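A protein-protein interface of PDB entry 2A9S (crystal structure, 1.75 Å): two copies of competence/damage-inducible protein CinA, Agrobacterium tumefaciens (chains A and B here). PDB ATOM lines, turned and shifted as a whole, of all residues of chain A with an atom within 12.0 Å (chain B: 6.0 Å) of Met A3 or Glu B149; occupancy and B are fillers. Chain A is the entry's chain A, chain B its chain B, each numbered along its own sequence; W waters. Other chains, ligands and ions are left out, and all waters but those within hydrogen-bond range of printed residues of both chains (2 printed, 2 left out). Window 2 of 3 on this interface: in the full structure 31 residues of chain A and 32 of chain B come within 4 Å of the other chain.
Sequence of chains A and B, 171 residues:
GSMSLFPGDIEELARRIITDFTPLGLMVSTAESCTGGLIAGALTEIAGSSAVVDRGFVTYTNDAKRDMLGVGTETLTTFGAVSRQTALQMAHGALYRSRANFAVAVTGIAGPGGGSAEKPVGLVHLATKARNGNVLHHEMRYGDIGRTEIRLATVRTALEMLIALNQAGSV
The side-chain hydroxyl (OG1) of Thr A44 is in hydrogen-bond range of the guanidinium group (NH1) of Arg B151, 3.0 Å away.
OG1 of Thr B148 is in hydrogen-bond range of OE1 of Glu A45 (2.6 Å).
The guanidinium group of Arg B151 lies within salt-bridge range of the side-chain carboxylate of Glu A45 (2.9 Å).
O of Thr A44 lies within hydrogen-bond range of NH2 of Arg B147, at 2.8 Å.
O of Gly A41 sits at hydrogen-bond distance from NH2 of Arg B151.
The backbone carbonyl oxygen (O) of Met A3 is in hydrogen-bond range of the side-chain hydroxyl (OG1) of Thr B148.
O of Gly A41 sits at hydrogen-bond distance from OG1 of Thr A44.
Among the printed residues, merely in contact across the chains: Met A3 with Glu B149 (3.6 Å), Glu A45 with Arg B147 (3.6 Å), Ile A46 with Arg B147 (3.6 Å) and Met A3 with Leu B152 (3.6 Å).
Met A3 touches three residues of chain B.
Glu B149 touches one residue of chain A.
Of chain A, only Met A3 and Glu A45 come within 4 Å of Thr B148.
No residue of chain A comes within 4 Å of Ile B150.
Of chain A, only Met A3 (3.6 Å) comes within 4 Å of Leu B152.
No residue of chain A comes within 4 Å of Ala B153.
Printed residues of chain B within 4 Å of Gly A41: Arg B151 (2.9 Å).
Of the printed residues of chain B, Ile A46 touches Arg B147 (3.6 Å).
Asp A9 touches none of the printed residues of chain B.
The nearest printed residue of chain B that does not touch Met A3 is Ile B145 (6.8 Å).
Printed residues of chain A that touch a printed residue of chain B: Met A3, Gly A41, Thr A44, Glu A45 and Ile A46.
No position is printed for both chains.
Of the 10 pairs that touch across the chains among the printed residues, none has its exchanged pair printed and touching as well.
Water W2 lies within hydrogen-bond range of OG1 of Thr B148 and O of Glu A45.
Water W1 bridges OE2 of Glu B149 and N of Met A3.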
ATOM      1  N   MET A   3     -36.754  19.186   3.883  1.00  0.00           N
ATOM      2  CA  MET A   3     -36.673  18.158   2.804  1.00  0.00           C
ATOM      3  C   MET A   3     -35.685  17.074   3.212  1.00  0.00           C
ATOM      4  O   MET A   3     -34.547  17.374   3.576  1.00  0.00           O
ATOM      5  CB  MET A   3     -36.199  18.796   1.489  1.00  0.00           C
ATOM      6  CG  MET A   3     -36.061  17.802   0.350  1.00  0.00           C
ATOM      7  SD  MET A   3     -35.499  18.559  -1.195  1.00  0.00           S
ATOM      8  CE  MET A   3     -35.591  17.133  -2.285  1.00  0.00           C
ATOM      9  N   SER A   4     -36.112  15.821   3.146  1.00  0.00           N
ATOM     10  CA  SER A   4     -35.234  14.710   3.519  1.00  0.00           C
ATOM     11  C   SER A   4     -34.604  14.111   2.252  1.00  0.00           C
ATOM     12  O   SER A   4     -35.236  14.116   1.176  1.00  0.00           O
ATOM     13  CB  SER A   4     -36.032  13.653   4.271  1.00  0.00           C
ATOM     14  OG  SER A   4     -35.305  13.176   5.396  1.00  0.00           O
ATOM     15  N   LEU A   5     -33.356  13.654   2.358  1.00  0.00           N
ATOM     16  CA  LEU A   5     -32.716  12.928   1.252  1.00  0.00           C
ATOM     17  C   LEU A   5     -32.470  11.495   1.699  1.00  0.00           C
ATOM     18  O   LEU A   5     -32.837  10.563   0.997  1.00  0.00           O
ATOM     19  CB  LEU A   5     -31.409  13.618   0.770  1.00  0.00           C
ATOM     20  CG  LEU A   5     -30.591  12.920  -0.329  1.00  0.00           C
ATOM     21  CD1 LEU A   5     -31.353  12.789  -1.664  1.00  0.00           C
ATOM     22  CD2 LEU A   5     -29.230  13.597  -0.580  1.00  0.00           C
ATOM     23  N   PHE A   6     -31.851  11.324   2.866  1.00  0.00           N
ATOM     24  CA  PHE A   6     -31.568   9.983   3.409  1.00  0.00           C
ATOM     25  C   PHE A   6     -32.712   9.444   4.262  1.00  0.00           C
ATOM     26  O   PHE A   6     -33.517  10.233   4.761  1.00  0.00           O
ATOM     27  CB  PHE A   6     -30.288   9.996   4.261  1.00  0.00           C
ATOM     28  CG  PHE A   6     -29.033  10.220   3.446  1.00  0.00           C
ATOM     29  CD1 PHE A   6     -28.335   9.132   2.933  1.00  0.00           C
ATOM     30  CD2 PHE A   6     -28.589  11.517   3.155  1.00  0.00           C
ATOM     31  CE1 PHE A   6     -27.181   9.355   2.146  1.00  0.00           C
ATOM     32  CE2 PHE A   6     -27.430  11.745   2.411  1.00  0.00           C
ATOM     33  CZ  PHE A   6     -26.737  10.646   1.908  1.00  0.00           C
ATOM     34  N   PRO A   7     -32.758   8.112   4.464  1.00  0.00           N
ATOM     35  CA  PRO A   7     -33.710   7.523   5.425  1.00  0.00           C
ATOM     36  C   PRO A   7     -33.635   8.196   6.805  1.00  0.00           C
ATOM     37  O   PRO A   7     -32.544   8.507   7.298  1.00  0.00           O
ATOM     38  CB  PRO A   7     -33.256   6.081   5.530  1.00  0.00           C
ATOM     39  CG  PRO A   7     -32.628   5.788   4.194  1.00  0.00           C
ATOM     40  CD  PRO A   7     -31.934   7.073   3.813  1.00  0.00           C
ATOM     41  N   GLY A   8     -34.797   8.390   7.425  1.00  0.00           N
ATOM     42  CA  GLY A   8     -34.921   9.076   8.705  1.00  0.00           C
ATOM     43  C   GLY A   8     -33.954   8.653   9.797  1.00  0.00           C
ATOM     44  O   GLY A   8     -33.408   9.515  10.516  1.00  0.00           O
ATOM     45  N   ASP A   9     -33.735   7.340   9.925  1.00  0.00           N
ATOM     46  CA  ASP A   9     -32.845   6.865  10.948  1.00  0.00           C
ATOM     47  C   ASP A   9     -31.369   7.233  10.659  1.00  0.00           C
ATOM     48  O   ASP A   9     -30.634   7.540  11.602  1.00  0.00           O
ATOM     49  CB  ASP A   9     -33.066   5.381  11.263  1.00  0.00           C
ATOM     50  CG  ASP A   9     -32.404   4.452  10.263  1.00  0.00           C
ATOM     51  OD1 ASP A   9     -32.689   4.540   9.038  1.00  0.00           O
ATOM     52  OD2 ASP A   9     -31.606   3.613  10.726  1.00  0.00           O
ATOM     53  N   ILE A  10     -30.965   7.225   9.374  1.00  0.00           N
ATOM     54  CA  ILE A  10     -29.618   7.662   8.965  1.00  0.00           C
ATOM     55  C   ILE A  10     -29.420   9.147   9.255  1.00  0.00           C
ATOM     56  O   ILE A  10     -28.402   9.536   9.869  1.00  0.00           O
ATOM     57  CB  ILE A  10     -29.321   7.343   7.492  1.00  0.00           C
ATOM     58  CG1 ILE A  10     -29.198   5.802   7.303  1.00  0.00           C
ATOM     59  CG2 ILE A  10     -28.081   8.121   6.992  1.00  0.00           C
ATOM     60  CD1 ILE A  10     -29.024   5.373   5.823  1.00  0.00           C
ATOM     61  N   GLU A  11     -30.400   9.967   8.857  1.00  0.00           N
ATOM     62  CA  GLU A  11     -30.395  11.374   9.230  1.00  0.00           C
ATOM     63  C   GLU A  11     -30.333  11.597  10.765  1.00  0.00           C
ATOM     64  O   GLU A  11     -29.547  12.454  11.240  1.00  0.00           O
ATOM     65  CB  GLU A  11     -31.596  12.073   8.649  1.00  0.00           C
ATOM     66  CG  GLU A  11     -31.503  13.541   8.778  1.00  0.00           C
ATOM     67  CD  GLU A  11     -32.805  14.203   8.448  1.00  0.00           C
ATOM     68  OE1 GLU A  11     -33.517  13.682   7.550  1.00  0.00           O
ATOM     69  OE2 GLU A  11     -33.109  15.239   9.086  1.00  0.00           O
ATOM     70  N   GLU A  12     -31.114  10.814  11.526  1.00  0.00           N
ATOM     71  CA  GLU A  12     -31.051  10.828  13.015  1.00  0.00           C
ATOM     72  C   GLU A  12     -29.627  10.550  13.507  1.00  0.00           C
ATOM     73  O   GLU A  12     -29.104  11.255  14.405  1.00  0.00           O
ATOM     74  CB  GLU A  12     -32.037   9.794  13.629  1.00  0.00           C
ATOM     75  CG  GLU A  12     -32.238   9.891  15.162  1.00  0.00           C
ATOM     76  CD  GLU A  12     -33.187   8.821  15.826  1.00  0.00           C
ATOM     77  OE1 GLU A  12     -33.332   7.641  15.342  1.00  0.00           O
ATOM     78  OE2 GLU A  12     -33.771   9.164  16.900  1.00  0.00           O
ATOM     79  N   ALA A  14     -26.706  10.845  11.830  1.00  0.00           N
ATOM     80  CA  ALA A  14     -25.855  11.960  11.433  1.00  0.00           C
ATOM     81  C   ALA A  14     -26.065  13.146  12.388  1.00  0.00           C
ATOM     82  O   ALA A  14     -25.097  13.779  12.864  1.00  0.00           O
ATOM     83  CB  ALA A  14     -26.134  12.348   9.956  1.00  0.00           C
ATOM     84  N   ARG A  15     -27.330  13.403  12.718  1.00  0.00           N
ATOM     85  CA  ARG A  15     -27.667  14.521  13.606  1.00  0.00           C
ATOM     86  C   ARG A  15     -27.047  14.287  14.978  1.00  0.00           C
ATOM     87  O   ARG A  15     -26.527  15.234  15.559  1.00  0.00           O
ATOM     88  CB  ARG A  15     -29.188  14.674  13.755  1.00  0.00           C
ATOM     89  CG  ARG A  15     -29.599  16.060  14.327  1.00  0.00           C
ATOM     90  CD  ARG A  15     -31.071  16.364  14.099  1.00  0.00           C
ATOM     91  NE  ARG A  15     -31.427  16.385  12.669  1.00  0.00           N
ATOM     92  CZ  ARG A  15     -31.162  17.389  11.827  1.00  0.00           C
ATOM     93  NH1 ARG A  15     -31.530  17.298  10.553  1.00  0.00           N
ATOM     94  NH2 ARG A  15     -30.540  18.488  12.237  1.00  0.00           N
ATOM     95  N   GLY A  41     -21.798  12.697   2.655  1.00  0.00           N
ATOM     96  CA  GLY A  41     -23.064  13.288   2.193  1.00  0.00           C
ATOM     97  C   GLY A  41     -24.097  13.321   3.327  1.00  0.00           C
ATOM     98  O   GLY A  41     -24.710  14.351   3.619  1.00  0.00           O
ATOM     99  N   ALA A  42     -24.266  12.181   3.983  1.00  0.00           N
ATOM    100  CA  ALA A  42     -25.197  12.070   5.094  1.00  0.00           C
ATOM    101  C   ALA A  42     -24.836  12.997   6.259  1.00  0.00           C
ATOM    102  O   ALA A  42     -25.691  13.697   6.763  1.00  0.00           O
ATOM    103  CB  ALA A  42     -25.350  10.623   5.546  1.00  0.00           C
ATOM    104  N   LEU A  43     -23.574  13.024   6.662  1.00  0.00           N
ATOM    105  CA  LEU A  43     -23.147  13.921   7.747  1.00  0.00           C
ATOM    106  C   LEU A  43     -23.392  15.397   7.419  1.00  0.00           C
ATOM    107  O   LEU A  43     -23.779  16.193   8.299  1.00  0.00           O
ATOM    108  CB  LEU A  43     -21.673  13.713   8.048  1.00  0.00           C
ATOM    109  CG  LEU A  43     -21.405  12.390   8.777  1.00  0.00           C
ATOM    110  CD1 LEU A  43     -19.933  12.058   8.600  1.00  0.00           C
ATOM    111  CD2 LEU A  43     -21.749  12.493  10.283  1.00  0.00           C
ATOM    112  N   THR A  44     -23.203  15.759   6.142  1.00  0.00           N
ATOM    113  CA  THR A  44     -23.271  17.171   5.779  1.00  0.00           C
ATOM    114  C   THR A  44     -24.708  17.583   5.419  1.00  0.00           C
ATOM    115  O   THR A  44     -24.958  18.733   5.072  1.00  0.00           O
ATOM    116  CB  THR A  44     -22.284  17.535   4.680  1.00  0.00           C
ATOM    117  OG1 THR A  44     -22.524  16.725   3.538  1.00  0.00           O
ATOM    118  CG2 THR A  44     -20.825  17.286   5.128  1.00  0.00           C
ATOM    119  N   GLU A  45     -25.664  16.659   5.534  1.00  0.00           N
ATOM    120  CA  GLU A  45     -27.090  17.048   5.510  1.00  0.00           C
ATOM    121  C   GLU A  45     -27.491  17.901   6.749  1.00  0.00           C
ATOM    122  O   GLU A  45     -28.466  18.660   6.711  1.00  0.00           O
ATOM    123  CB  GLU A  45     -27.977  15.801   5.404  1.00  0.00           C
ATOM    124  CG  GLU A  45     -28.056  15.256   3.970  1.00  0.00           C
ATOM    125  CD  GLU A  45     -28.819  16.218   3.035  1.00  0.00           C
ATOM    126  OE1 GLU A  45     -30.082  16.361   3.163  1.00  0.00           O
ATOM    127  OE2 GLU A  45     -28.156  16.800   2.158  1.00  0.00           O
ATOM    128  N   ILE A  46     -26.709  17.792   7.817  1.00  0.00           N
ATOM    129  CA  ILE A  46     -27.002  18.427   9.092  1.00  0.00           C
ATOM    130  C   ILE A  46     -26.438  19.855   9.206  1.00  0.00           C
ATOM    131  O   ILE A  46     -25.225  20.087   9.040  1.00  0.00           O
ATOM    132  CB  ILE A  46     -26.466  17.544  10.234  1.00  0.00           C
ATOM    133  CG1 ILE A  46     -26.916  16.069  10.049  1.00  0.00           C
ATOM    134  CG2 ILE A  46     -26.776  18.164  11.619  1.00  0.00           C
ATOM    135  CD1 ILE A  46     -28.395  15.845  10.043  1.00  0.00           C
ATOM    136  N   ALA A  47     -27.323  20.815   9.471  1.00  0.00           N
ATOM    137  CA  ALA A  47     -26.873  22.177   9.708  1.00  0.00           C
ATOM    138  C   ALA A  47     -25.964  22.190  10.942  1.00  0.00           C
ATOM    139  O   ALA A  47     -26.270  21.565  11.962  1.00  0.00           O
ATOM    140  CB  ALA A  47     -28.053  23.133   9.867  1.00  0.00           C
ATOM    141  N   ILE B 145     -33.342  28.520  -0.729  1.00  0.00           N
ATOM    142  CA  ILE B 145     -34.358  27.541  -1.073  1.00  0.00           C
ATOM    143  C   ILE B 145     -34.275  26.252  -0.231  1.00  0.00           C
ATOM    144  O   ILE B 145     -35.099  25.324  -0.406  1.00  0.00           O
ATOM    145  CB  ILE B 145     -34.339  27.167  -2.611  1.00  0.00           C
ATOM    146  CG1 ILE B 145     -33.012  26.500  -3.028  1.00  0.00           C
ATOM    147  CG2 ILE B 145     -34.680  28.390  -3.510  1.00  0.00           C
ATOM    148  CD1 ILE B 145     -32.975  26.067  -4.508  1.00  0.00           C
ATOM    149  N   GLY B 146     -33.313  26.206   0.693  1.00  0.00           N
ATOM    150  CA  GLY B 146     -33.152  25.060   1.597  1.00  0.00           C
ATOM    151  C   GLY B 146     -31.821  24.350   1.367  1.00  0.00           C
ATOM    152  O   GLY B 146     -31.285  24.297   0.240  1.00  0.00           O
ATOM    153  N   ARG B 147     -31.276  23.776   2.436  1.00  0.00           N
ATOM    154  CA  ARG B 147     -29.914  23.212   2.358  1.00  0.00           C
ATOM    155  C   ARG B 147     -29.862  22.009   1.385  1.00  0.00           C
ATOM    156  O   ARG B 147     -29.024  21.966   0.483  1.00  0.00           O
ATOM    157  CB  ARG B 147     -29.445  22.861   3.780  1.00  0.00           C
ATOM    158  CG  ARG B 147     -28.039  22.301   3.811  1.00  0.00           C
ATOM    159  CD  ARG B 147     -27.721  21.832   5.215  1.00  0.00           C
ATOM    160  NE  ARG B 147     -26.369  21.279   5.304  1.00  0.00           N
ATOM    161  CZ  ARG B 147     -25.304  21.941   5.743  1.00  0.00           C
ATOM    162  NH1 ARG B 147     -25.400  23.222   6.109  1.00  0.00           N
ATOM    163  NH2 ARG B 147     -24.123  21.323   5.818  1.00  0.00           N
ATOM    164  N   THR B 148     -30.760  21.049   1.555  1.00  0.00           N
ATOM    165  CA  THR B 148     -30.803  19.865   0.664  1.00  0.00           C
ATOM    166  C   THR B 148     -31.089  20.309  -0.771  1.00  0.00           C
ATOM    167  O   THR B 148     -30.449  19.819  -1.721  1.00  0.00           O
ATOM    168  CB  THR B 148     -31.831  18.853   1.147  1.00  0.00           C
ATOM    169  OG1 THR B 148     -31.506  18.463   2.483  1.00  0.00           O
ATOM    170  CG2 THR B 148     -31.830  17.587   0.255  1.00  0.00           C
ATOM    171  N   GLU B 149     -32.029  21.254  -0.917  1.00  0.00           N
ATOM    172  CA  GLU B 149     -32.411  21.801  -2.233  1.00  0.00           C
ATOM    173  C   GLU B 149     -31.226  22.387  -2.971  1.00  0.00           C
ATOM    174  O   GLU B 149     -31.053  22.081  -4.156  1.00  0.00           O
ATOM    175  CB  GLU B 149     -33.551  22.842  -2.116  1.00  0.00           C
ATOM    176  CG  GLU B 149     -34.888  22.222  -1.653  1.00  0.00           C
ATOM    177  CD  GLU B 149     -35.108  22.152  -0.121  1.00  0.00           C
ATOM    178  OE1 GLU B 149     -34.164  22.085   0.688  1.00  0.00           O
ATOM    179  OE2 GLU B 149     -36.285  22.160   0.318  1.00  0.00           O
ATOM    180  N   ILE B 150     -30.428  23.226  -2.286  1.00  0.00           N
ATOM    181  CA  ILE B 150     -29.226  23.818  -2.927  1.00  0.00           C
ATOM    182  C   ILE B 150     -28.189  22.718  -3.305  1.00  0.00           C
ATOM    183  O   ILE B 150     -27.619  22.726  -4.398  1.00  0.00           O
ATOM    184  CB  ILE B 150     -28.616  24.922  -2.019  1.00  0.00           C
ATOM    185  CG1 ILE B 150     -29.613  26.092  -1.897  1.00  0.00           C
ATOM    186  CG2 ILE B 150     -27.255  25.333  -2.526  1.00  0.00           C
ATOM    187  CD1 ILE B 150     -29.327  27.066  -0.732  1.00  0.00           C
ATOM    188  N   ARG B 151     -27.970  21.787  -2.385  1.00  0.00           N
ATOM    189  CA  ARG B 151     -27.054  20.672  -2.657  1.00  0.00           C
ATOM    190  C   ARG B 151     -27.464  19.838  -3.910  1.00  0.00           C
ATOM    191  O   ARG B 151     -26.642  19.544  -4.792  1.00  0.00           O
ATOM    192  CB  ARG B 151     -26.915  19.843  -1.393  1.00  0.00           C
ATOM    193  CG  ARG B 151     -26.006  20.564  -0.423  1.00  0.00           C
ATOM    194  CD  ARG B 151     -26.217  20.150   1.026  1.00  0.00           C
ATOM    195  NE  ARG B 151     -26.203  18.729   1.322  1.00  0.00           N
ATOM    196  CZ  ARG B 151     -25.129  18.037   1.711  1.00  0.00           C
ATOM    197  NH1 ARG B 151     -23.937  18.641   1.761  1.00  0.00           N
ATOM    198  NH2 ARG B 151     -25.252  16.736   2.030  1.00  0.00           N
ATOM    199  N   LEU B 152     -28.739  19.513  -3.999  1.00  0.00           N
ATOM    200  CA  LEU B 152     -29.204  18.758  -5.155  1.00  0.00           C
ATOM    201  C   LEU B 152     -29.159  19.611  -6.432  1.00  0.00           C
ATOM    202  O   LEU B 152     -28.811  19.103  -7.480  1.00  0.00           O
ATOM    203  CB  LEU B 152     -30.607  18.248  -4.893  1.00  0.00           C
ATOM    204  CG  LEU B 152     -30.727  17.181  -3.797  1.00  0.00           C
ATOM    205  CD1 LEU B 152     -32.212  16.833  -3.623  1.00  0.00           C
ATOM    206  CD2 LEU B 152     -29.923  15.918  -4.153  1.00  0.00           C
ATOM    207  N   ALA B 153     -29.508  20.900  -6.332  1.00  0.00           N
ATOM    208  CA  ALA B 153     -29.409  21.802  -7.483  1.00  0.00           C
ATOM    209  C   ALA B 153     -27.986  21.838  -7.996  1.00  0.00           C
ATOM    210  O   ALA B 153     -27.763  21.798  -9.188  1.00  0.00           O
ATOM    211  CB  ALA B 153     -29.871  23.224  -7.121  1.00  0.00           C
ATOM    212  N   THR B 154     -27.031  21.859  -7.059  1.00  0.00           N
ATOM    213  CA  THR B 154     -25.611  21.921  -7.388  1.00  0.00           C
ATOM    214  C   THR B 154     -25.165  20.627  -8.059  1.00  0.00           C
ATOM    215  O   THR B 154     -24.423  20.666  -9.076  1.00  0.00           O
ATOM    216  CB  THR B 154     -24.771  22.177  -6.108  1.00  0.00           C
ATOM    217  OG1 THR B 154     -25.124  23.468  -5.584  1.00  0.00           O
ATOM    218  CG2 THR B 154     -23.259  22.155  -6.434  1.00  0.00           C
HETATM  219  O   HOH W   1     -36.832  21.913   3.026  1.00  0.00           O
HETATM  220  O   HOH W   2     -29.645  19.153   4.098  1.00  0.00           O
